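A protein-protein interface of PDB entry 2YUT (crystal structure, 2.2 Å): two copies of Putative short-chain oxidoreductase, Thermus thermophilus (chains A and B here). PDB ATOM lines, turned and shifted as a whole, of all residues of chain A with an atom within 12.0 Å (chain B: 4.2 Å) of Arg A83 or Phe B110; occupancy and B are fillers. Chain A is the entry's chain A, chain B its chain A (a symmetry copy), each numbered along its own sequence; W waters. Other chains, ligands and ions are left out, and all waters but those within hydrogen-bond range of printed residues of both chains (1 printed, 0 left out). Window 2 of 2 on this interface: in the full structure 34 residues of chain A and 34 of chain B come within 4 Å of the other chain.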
ATOM      1  N   ARG A  79     -13.451  21.636   6.146  1.00  0.00           N
ATOM      2  CA  ARG A  79     -14.055  22.933   6.420  1.00  0.00           C
ATOM      3  C   ARG A  79     -15.515  22.758   6.814  1.00  0.00           C
ATOM      4  O   ARG A  79     -16.252  22.021   6.163  1.00  0.00           O
ATOM      5  CB  ARG A  79     -13.966  23.832   5.183  1.00  0.00           C
ATOM      6  CG  ARG A  79     -14.720  25.148   5.328  1.00  0.00           C
ATOM      7  CD  ARG A  79     -14.738  25.939   4.031  1.00  0.00           C
ATOM      8  NE  ARG A  79     -13.423  26.469   3.685  1.00  0.00           N
ATOM      9  CZ  ARG A  79     -12.795  26.219   2.541  1.00  0.00           C
ATOM     10  NH1 ARG A  79     -13.362  25.442   1.626  1.00  0.00           N
ATOM     11  NH2 ARG A  79     -11.603  26.753   2.306  1.00  0.00           N
ATOM     12  N   ALA A  80     -15.926  23.431   7.883  1.00  0.00           N
ATOM     13  CA  ALA A  80     -17.308  23.360   8.349  1.00  0.00           C
ATOM     14  C   ALA A  80     -17.565  24.372   9.457  1.00  0.00           C
ATOM     15  O   ALA A  80     -16.654  24.744  10.194  1.00  0.00           O
ATOM     16  CB  ALA A  80     -17.623  21.965   8.844  1.00  0.00           C
ATOM     17  N   SER A  81     -18.807  24.832   9.557  1.00  0.00           N
ATOM     18  CA  SER A  81     -19.165  25.781  10.603  1.00  0.00           C
ATOM     19  C   SER A  81     -19.428  24.959  11.855  1.00  0.00           C
ATOM     20  O   SER A  81     -19.658  23.749  11.776  1.00  0.00           O
ATOM     21  CB  SER A  81     -20.431  26.550  10.228  1.00  0.00           C
ATOM     22  OG  SER A  81     -21.564  25.702  10.263  1.00  0.00           O
ATOM     23  N   VAL A  82     -19.393  25.607  13.011  1.00  0.00           N
ATOM     24  CA  VAL A  82     -19.640  24.906  14.263  1.00  0.00           C
ATOM     25  C   VAL A  82     -21.129  24.905  14.579  1.00  0.00           C
ATOM     26  O   VAL A  82     -21.579  24.221  15.497  1.00  0.00           O
ATOM     27  CB  VAL A  82     -18.898  25.575  15.434  1.00  0.00           C
ATOM     28  CG1 VAL A  82     -17.409  25.629  15.139  1.00  0.00           C
ATOM     29  CG2 VAL A  82     -19.453  26.974  15.670  1.00  0.00           C
ATOM     30  N   ARG A  83     -21.891  25.671  13.805  1.00  0.00           N
ATOM     31  CA  ARG A  83     -23.325  25.788  14.025  1.00  0.00           C
ATOM     32  C   ARG A  83     -24.174  24.841  13.188  1.00  0.00           C
ATOM     33  O   ARG A  83     -25.366  24.684  13.450  1.00  0.00           O
ATOM     34  CB  ARG A  83     -23.754  27.238  13.788  1.00  0.00           C
ATOM     35  CG  ARG A  83     -23.139  28.200  14.794  1.00  0.00           C
ATOM     36  CD  ARG A  83     -23.745  27.984  16.176  1.00  0.00           C
ATOM     37  NE  ARG A  83     -25.050  28.626  16.295  1.00  0.00           N
ATOM     38  CZ  ARG A  83     -25.985  28.274  17.172  1.00  0.00           C
ATOM     39  NH1 ARG A  83     -25.767  27.270  18.011  1.00  0.00           N
ATOM     40  NH2 ARG A  83     -27.135  28.933  17.219  1.00  0.00           N
ATOM     41  N   GLU A  84     -23.570  24.209  12.186  1.00  0.00           N
ATOM     42  CA  GLU A  84     -24.300  23.272  11.340  1.00  0.00           C
ATOM     43  C   GLU A  84     -23.366  22.275  10.665  1.00  0.00           C
ATOM     44  O   GLU A  84     -23.732  21.117  10.458  1.00  0.00           O
ATOM     45  CB  GLU A  84     -25.101  24.023  10.274  1.00  0.00           C
ATOM     46  CG  GLU A  84     -24.252  24.801   9.284  1.00  0.00           C
ATOM     47  CD  GLU A  84     -25.082  25.459   8.197  1.00  0.00           C
ATOM     48  OE1 GLU A  84     -24.493  26.125   7.320  1.00  0.00           O
ATOM     49  OE2 GLU A  84     -26.322  25.308   8.220  1.00  0.00           O
ATOM     50  N   ASP A  88     -19.320  14.731  12.027  1.00  0.00           N
ATOM     51  CA  ASP A  88     -18.324  14.169  12.930  1.00  0.00           C
ATOM     52  C   ASP A  88     -16.936  14.690  12.577  1.00  0.00           C
ATOM     53  O   ASP A  88     -15.940  13.999  12.785  1.00  0.00           O
ATOM     54  CB  ASP A  88     -18.320  12.643  12.833  1.00  0.00           C
ATOM     55  CG  ASP A  88     -19.703  12.046  12.966  1.00  0.00           C
ATOM     56  OD1 ASP A  88     -20.369  12.305  13.992  1.00  0.00           O
ATOM     57  OD2 ASP A  88     -20.122  11.316  12.043  1.00  0.00           O
ATOM     58  N   LEU A  89     -16.879  15.907  12.044  1.00  0.00           N
ATOM     59  CA  LEU A  89     -15.613  16.514  11.645  1.00  0.00           C
ATOM     60  C   LEU A  89     -14.650  16.705  12.817  1.00  0.00           C
ATOM     61  O   LEU A  89     -13.457  16.433  12.691  1.00  0.00           O
ATOM     62  CB  LEU A  89     -15.866  17.862  10.960  1.00  0.00           C
ATOM     63  CG  LEU A  89     -14.648  18.551  10.336  1.00  0.00           C
ATOM     64  CD1 LEU A  89     -14.102  17.701   9.207  1.00  0.00           C
ATOM     65  CD2 LEU A  89     -15.038  19.917   9.811  1.00  0.00           C
ATOM     66  N   VAL A  90     -15.167  17.170  13.953  1.00  0.00           N
ATOM     67  CA  VAL A  90     -14.326  17.390  15.124  1.00  0.00           C
ATOM     68  C   VAL A  90     -13.649  16.095  15.575  1.00  0.00           C
ATOM     69  O   VAL A  90     -12.446  16.070  15.826  1.00  0.00           O
ATOM     70  CB  VAL A  90     -15.139  17.979  16.303  1.00  0.00           C
ATOM     71  CG1 VAL A  90     -14.251  18.126  17.534  1.00  0.00           C
ATOM     72  CG2 VAL A  90     -15.699  19.336  15.911  1.00  0.00           C
ATOM     73  N   VAL A 128      -9.862  30.400  12.404  1.00  0.00           N
ATOM     74  CA  VAL A 128     -10.755  31.256  11.636  1.00  0.00           C
ATOM     75  C   VAL A 128     -12.010  30.479  11.247  1.00  0.00           C
ATOM     76  O   VAL A 128     -12.025  29.247  11.281  1.00  0.00           O
ATOM     77  CB  VAL A 128     -10.063  31.754  10.340  1.00  0.00           C
ATOM     78  CG1 VAL A 128      -8.713  32.370  10.671  1.00  0.00           C
ATOM     79  CG2 VAL A 128      -9.885  30.597   9.363  1.00  0.00           C
ATOM     80  N   PRO A 129     -13.079  31.195  10.862  1.00  0.00           N
ATOM     81  CA  PRO A 129     -14.346  30.574  10.463  1.00  0.00           C
ATOM     82  C   PRO A 129     -14.161  29.459   9.438  1.00  0.00           C
ATOM     83  O   PRO A 129     -13.463  29.629   8.438  1.00  0.00           O
ATOM     84  CB  PRO A 129     -15.137  31.748   9.897  1.00  0.00           C
ATOM     85  CG  PRO A 129     -14.667  32.894  10.750  1.00  0.00           C
ATOM     86  CD  PRO A 129     -13.174  32.666  10.800  1.00  0.00           C
ATOM     87  N   GLY A 130     -14.793  28.319   9.698  1.00  0.00           N
ATOM     88  CA  GLY A 130     -14.697  27.195   8.788  1.00  0.00           C
ATOM     89  C   GLY A 130     -13.671  26.151   9.186  1.00  0.00           C
ATOM     90  O   GLY A 130     -13.795  24.993   8.795  1.00  0.00           O
ATOM     91  N   PHE A 131     -12.672  26.544   9.975  1.00  0.00           N
ATOM     92  CA  PHE A 131     -11.624  25.614  10.386  1.00  0.00           C
ATOM     93  C   PHE A 131     -11.542  25.316  11.885  1.00  0.00           C
ATOM     94  O   PHE A 131     -10.489  24.914  12.378  1.00  0.00           O
ATOM     95  CB  PHE A 131     -10.265  26.128   9.905  1.00  0.00           C
ATOM     96  CG  PHE A 131     -10.142  26.209   8.410  1.00  0.00           C
ATOM     97  CD1 PHE A 131     -10.482  25.122   7.612  1.00  0.00           C
ATOM     98  CD2 PHE A 131      -9.669  27.366   7.799  1.00  0.00           C
ATOM     99  CE1 PHE A 131     -10.354  25.185   6.226  1.00  0.00           C
ATOM    100  CE2 PHE A 131      -9.535  27.442   6.414  1.00  0.00           C
ATOM    101  CZ  PHE A 131      -9.879  26.347   5.627  1.00  0.00           C
ATOM    102  N   ALA A 132     -12.646  25.492  12.604  1.00  0.00           N
ATOM    103  CA  ALA A 132     -12.657  25.239  14.043  1.00  0.00           C
ATOM    104  C   ALA A 132     -12.166  23.833  14.388  1.00  0.00           C
ATOM    105  O   ALA A 132     -11.309  23.661  15.253  1.00  0.00           O
ATOM    106  CB  ALA A 132     -14.058  25.447  14.598  1.00  0.00           C
ATOM    107  N   ALA A 133     -12.708  22.830  13.708  1.00  0.00           N
ATOM    108  CA  ALA A 133     -12.311  21.451  13.964  1.00  0.00           C
ATOM    109  C   ALA A 133     -10.799  21.266  13.768  1.00  0.00           C
ATOM    110  O   ALA A 133     -10.113  20.754  14.653  1.00  0.00           O
ATOM    111  CB  ALA A 133     -13.093  20.509  13.056  1.00  0.00           C
ATOM    112  N   LEU B  67     -31.495  30.964  24.559  1.00  0.00           N
ATOM    113  CA  LEU B  67     -30.760  31.309  25.769  1.00  0.00           C
ATOM    114  C   LEU B  67     -30.146  32.705  25.709  1.00  0.00           C
ATOM    115  O   LEU B  67     -29.782  33.192  24.634  1.00  0.00           O
ATOM    116  CB  LEU B  67     -29.627  30.298  25.997  1.00  0.00           C
ATOM    117  CG  LEU B  67     -29.949  28.796  26.047  1.00  0.00           C
ATOM    118  CD1 LEU B  67     -28.644  28.005  26.060  1.00  0.00           C
ATOM    119  CD2 LEU B  67     -30.782  28.471  27.281  1.00  0.00           C
ATOM    120  N   LEU B  70     -25.181  30.990  28.588  1.00  0.00           N
ATOM    121  CA  LEU B  70     -24.798  29.586  28.689  1.00  0.00           C
ATOM    122  C   LEU B  70     -23.471  29.518  29.435  1.00  0.00           C
ATOM    123  O   LEU B  70     -22.528  30.240  29.107  1.00  0.00           O
ATOM    124  CB  LEU B  70     -24.627  28.967  27.295  1.00  0.00           C
ATOM    125  CG  LEU B  70     -23.888  27.624  27.213  1.00  0.00           C
ATOM    126  CD1 LEU B  70     -24.742  26.508  27.815  1.00  0.00           C
ATOM    127  CD2 LEU B  70     -23.567  27.310  25.754  1.00  0.00           C
ATOM    128  N   LEU B 105     -22.609  23.800  21.693  1.00  0.00           N
ATOM    129  CA  LEU B 105     -22.523  25.004  20.879  1.00  0.00           C
ATOM    130  C   LEU B 105     -23.201  24.862  19.518  1.00  0.00           C
ATOM    131  O   LEU B 105     -23.736  25.828  18.976  1.00  0.00           O
ATOM    132  CB  LEU B 105     -21.055  25.397  20.689  1.00  0.00           C
ATOM    133  CG  LEU B 105     -20.790  26.720  19.970  1.00  0.00           C
ATOM    134  CD1 LEU B 105     -21.506  27.855  20.704  1.00  0.00           C
ATOM    135  CD2 LEU B 105     -19.292  26.981  19.906  1.00  0.00           C
ATOM    136  N   LYS B 106     -23.180  23.658  18.966  1.00  0.00           N
ATOM    137  CA  LYS B 106     -23.792  23.426  17.669  1.00  0.00           C
ATOM    138  C   LYS B 106     -25.316  23.461  17.695  1.00  0.00           C
ATOM    139  O   LYS B 106     -25.941  24.004  16.791  1.00  0.00           O
ATOM    140  CB  LYS B 106     -23.344  22.073  17.108  1.00  0.00           C
ATOM    141  CG  LYS B 106     -24.049  21.681  15.806  1.00  0.00           C
ATOM    142  CD  LYS B 106     -23.609  20.301  15.320  1.00  0.00           C
ATOM    143  CE  LYS B 106     -24.294  19.926  14.011  1.00  0.00           C
ATOM    144  NZ  LYS B 106     -23.974  18.533  13.594  1.00  0.00           N
ATOM    145  N   ALA B 108     -27.267  24.701  20.366  1.00  0.00           N
ATOM    146  CA  ALA B 108     -27.852  25.727  21.220  1.00  0.00           C
ATOM    147  C   ALA B 108     -28.668  26.784  20.472  1.00  0.00           C
ATOM    148  O   ALA B 108     -28.324  27.201  19.365  1.00  0.00           O
ATOM    149  CB  ALA B 108     -26.755  26.408  22.033  1.00  0.00           C
ATOM    150  N   ARG B 109     -29.766  27.202  21.084  1.00  0.00           N
ATOM    151  CA  ARG B 109     -30.596  28.260  20.518  1.00  0.00           C
ATOM    152  C   ARG B 109     -30.193  29.497  21.315  1.00  0.00           C
ATOM    153  O   ARG B 109     -30.167  29.454  22.544  1.00  0.00           O
ATOM    154  CB  ARG B 109     -32.079  27.975  20.746  1.00  0.00           C
ATOM    155  CG  ARG B 109     -32.742  27.105  19.695  1.00  0.00           C
ATOM    156  CD  ARG B 109     -32.142  25.719  19.621  1.00  0.00           C
ATOM    157  NE  ARG B 109     -33.014  24.821  18.869  1.00  0.00           N
ATOM    158  CZ  ARG B 109     -32.631  23.659  18.354  1.00  0.00           C
ATOM    159  NH1 ARG B 109     -31.381  23.243  18.503  1.00  0.00           N
ATOM    160  NH2 ARG B 109     -33.501  22.913  17.688  1.00  0.00           N
ATOM    161  N   PHE B 110     -29.874  30.587  20.627  1.00  0.00           N
ATOM    162  CA  PHE B 110     -29.453  31.814  21.298  1.00  0.00           C
ATOM    163  C   PHE B 110     -30.286  33.033  20.942  1.00  0.00           C
ATOM    164  O   PHE B 110     -30.761  33.165  19.818  1.00  0.00           O
ATOM    165  CB  PHE B 110     -27.999  32.151  20.944  1.00  0.00           C
ATOM    166  CG  PHE B 110     -26.983  31.222  21.543  1.00  0.00           C
ATOM    167  CD1 PHE B 110     -26.773  31.189  22.917  1.00  0.00           C
ATOM    168  CD2 PHE B 110     -26.202  30.408  20.723  1.00  0.00           C
ATOM    169  CE1 PHE B 110     -25.796  30.362  23.470  1.00  0.00           C
ATOM    170  CE2 PHE B 110     -25.221  29.574  21.264  1.00  0.00           C
ATOM    171  CZ  PHE B 110     -25.017  29.551  22.641  1.00  0.00           C
ATOM    172  N   GLN B 111     -30.442  33.928  21.913  1.00  0.00           N
ATOM    173  CA  GLN B 111     -31.148  35.191  21.714  1.00  0.00           C
ATOM    174  C   GLN B 111     -30.039  36.119  21.218  1.00  0.00           C
ATOM    175  O   GLN B 111     -28.863  35.869  21.492  1.00  0.00           O
ATOM    176  CB  GLN B 111     -31.670  35.742  23.049  1.00  0.00           C
ATOM    177  CG  GLN B 111     -32.780  34.933  23.698  1.00  0.00           C
ATOM    178  CD  GLN B 111     -34.133  35.215  23.082  1.00  0.00           C
ATOM    179  OE1 GLN B 111     -34.221  35.722  21.960  1.00  0.00           O
ATOM    180  NE2 GLN B 111     -35.197  34.874  23.803  1.00  0.00           N
ATOM    181  N   LYS B 112     -30.390  37.171  20.491  1.00  0.00           N
ATOM    182  CA  LYS B 112     -29.372  38.117  20.040  1.00  0.00           C
ATOM    183  C   LYS B 112     -28.771  38.703  21.315  1.00  0.00           C
ATOM    184  O   LYS B 112     -29.487  38.940  22.286  1.00  0.00           O
ATOM    185  CB  LYS B 112     -30.000  39.237  19.204  1.00  0.00           C
ATOM    186  CG  LYS B 112     -30.488  38.804  17.824  1.00  0.00           C
ATOM    187  CD  LYS B 112     -29.320  38.461  16.909  1.00  0.00           C
ATOM    188  CE  LYS B 112     -29.790  38.032  15.525  1.00  0.00           C
ATOM    189  NZ  LYS B 112     -30.521  39.120  14.816  1.00  0.00           N
ATOM    190  N   ALA B 114     -26.780  37.191  23.349  1.00  0.00           N
ATOM    191  CA  ALA B 114     -26.439  36.154  24.315  1.00  0.00           C
ATOM    192  C   ALA B 114     -24.933  35.975  24.488  1.00  0.00           C
ATOM    193  O   ALA B 114     -24.137  36.335  23.615  1.00  0.00           O
ATOM    194  CB  ALA B 114     -27.065  34.835  23.898  1.00  0.00           C
ATOM    195  N   ALA B 116     -21.969  33.053  25.774  1.00  0.00           N
ATOM    196  CA  ALA B 116     -21.745  31.629  25.975  1.00  0.00           C
ATOM    197  C   ALA B 116     -20.353  31.527  26.575  1.00  0.00           C
ATOM    198  O   ALA B 116     -19.355  31.879  25.939  1.00  0.00           O
ATOM    199  CB  ALA B 116     -21.836  30.884  24.646  1.00  0.00           C
ATOM    200  N   LEU B 152     -20.211  32.952  15.499  1.00  0.00           N
ATOM    201  CA  LEU B 152     -21.239  33.239  16.492  1.00  0.00           C
ATOM    202  C   LEU B 152     -21.599  34.718  16.579  1.00  0.00           C
ATOM    203  O   LEU B 152     -22.765  35.068  16.759  1.00  0.00           O
ATOM    204  CB  LEU B 152     -20.792  32.721  17.864  1.00  0.00           C
ATOM    205  CG  LEU B 152     -21.018  31.226  18.122  1.00  0.00           C
ATOM    206  CD1 LEU B 152     -22.513  30.964  18.284  1.00  0.00           C
ATOM    207  CD2 LEU B 152     -20.449  30.389  16.976  1.00  0.00           C
ATOM    208  N   GLU B 155     -24.326  35.875  14.583  1.00  0.00           N
ATOM    209  CA  GLU B 155     -25.661  35.576  15.093  1.00  0.00           C
ATOM    210  C   GLU B 155     -25.967  36.487  16.276  1.00  0.00           C
ATOM    211  O   GLU B 155     -27.018  36.366  16.901  1.00  0.00           O
ATOM    212  CB  GLU B 155     -25.753  34.119  15.562  1.00  0.00           C
ATOM    213  CG  GLU B 155     -25.600  33.076  14.476  1.00  0.00           C
ATOM    214  CD  GLU B 155     -25.758  31.662  15.011  1.00  0.00           C
ATOM    215  OE1 GLU B 155     -26.820  31.351  15.590  1.00  0.00           O
ATOM    216  OE2 GLU B 155     -24.817  30.859  14.857  1.00  0.00           O
ATOM    217  N   VAL B 157     -24.096  36.566  18.966  1.00  0.00           N
ATOM    218  CA  VAL B 157     -23.707  35.826  20.160  1.00  0.00           C
ATOM    219  C   VAL B 157     -22.234  36.026  20.504  1.00  0.00           C
ATOM    220  O   VAL B 157     -21.360  35.908  19.642  1.00  0.00           O
ATOM    221  CB  VAL B 157     -23.970  34.320  19.975  1.00  0.00           C
ATOM    222  CG1 VAL B 157     -23.578  33.563  21.232  1.00  0.00           C
ATOM    223  CG2 VAL B 157     -25.431  34.093  19.648  1.00  0.00           C
HETATM  224  O   HOH W   1     -29.903  30.405  17.776  1.00  0.00           O
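The backbone carbonyl oxygen of Leu B105 lies within hydrogen-bond range of the guanidinium group of Arg A83.
The guanidinium group (NH1) of Arg A83 lies within hydrogen-bond range of the backbone carbonyl oxygen (O) of Lys B106 (3.5 Å).
The backbone carbonyl oxygen (O) of Ala B108 sits at hydrogen-bond distance from the guanidinium group (NH1) of Arg A83 (2.9 Å).
NE of Arg A83 lies within salt-bridge range of OE2 of Glu B155, 2.7 Å away.
OG of Ser A81 sits close to N of Glu A84 (3.2 Å).
The backbone carbonyl oxygen of Leu B152 lies within hydrogen-bond range of the backbone NH of Val B157, 3.0 Å away.
O of Val A82 touches CA of Lys B106 (3.2 Å).
Val A82 touches Leu B152 (CG2 to CD2, 3.8 Å).
NH2 of Arg A83 touches CD2 of Phe B110, 3.9 Å away.
CD1 of Leu B152 touches CD of Arg A83, at 3.9 Å.
CE of Lys B106 touches O of Glu A84 (3.8 Å).
Arg A83 touches six residues of chain B.
Of chain A, only Arg A83 (3.9 Å) comes within 4 Å of Phe B110.
Leu B67 touches none of the printed residues of chain A.
No residue of chain A comes within 4 Å of Leu B70.
Leu B105 touches just one residue of chain A: Arg A83 (2.7 Å).
Of chain A, only Val A82 (3.2 Å), Arg A83 (3.5 Å) and Glu A84 (3.8 Å) come within 4 Å of Lys B106.
No residue of chain A comes within 4 Å of Gln B111.
No residue of chain A comes within 4 Å of Ala B116.
Leu B152 touches just these residues of chain A: Val A82 (3.8 Å) and Arg A83 (3.9 Å).
Of chain A, only Arg A83 comes within 4 Å of Glu B155.
Of the printed residues of chain B, Val A82 touches Lys B106 and Leu B152.
Of the printed residues of chain B, Glu A84 touches Lys B106 (3.8 Å).
The nearest residue of chain A that does not touch Phe B110 is Val A82 (8.4 Å).
The nearest printed residue of chain B that does not touch Val A82 is Leu B105 (4.2 Å).
Hydrophobic or aromatic side chains of chain B that line the printed part of chain A: Phe B110 and Leu B152.
Hydrophobic or aromatic side chains of chain A within 4 Å of the printed part of chain B: Val A82.
Among the printed residues, Asp or Glu carboxylates within 4 Å of a Lys or Arg side-chain nitrogen of the other chain: Arg A83 with Glu B155.
No position is printed for both chains.
Of the 9 pairs that touch across the chains among the printed residues, none has its exchanged pair printed and touching as well.
Water W1 bridges the backbone NH of Phe B110 (2.9 Å) and the guanidinium group of Arg A83 (3.2 Å).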
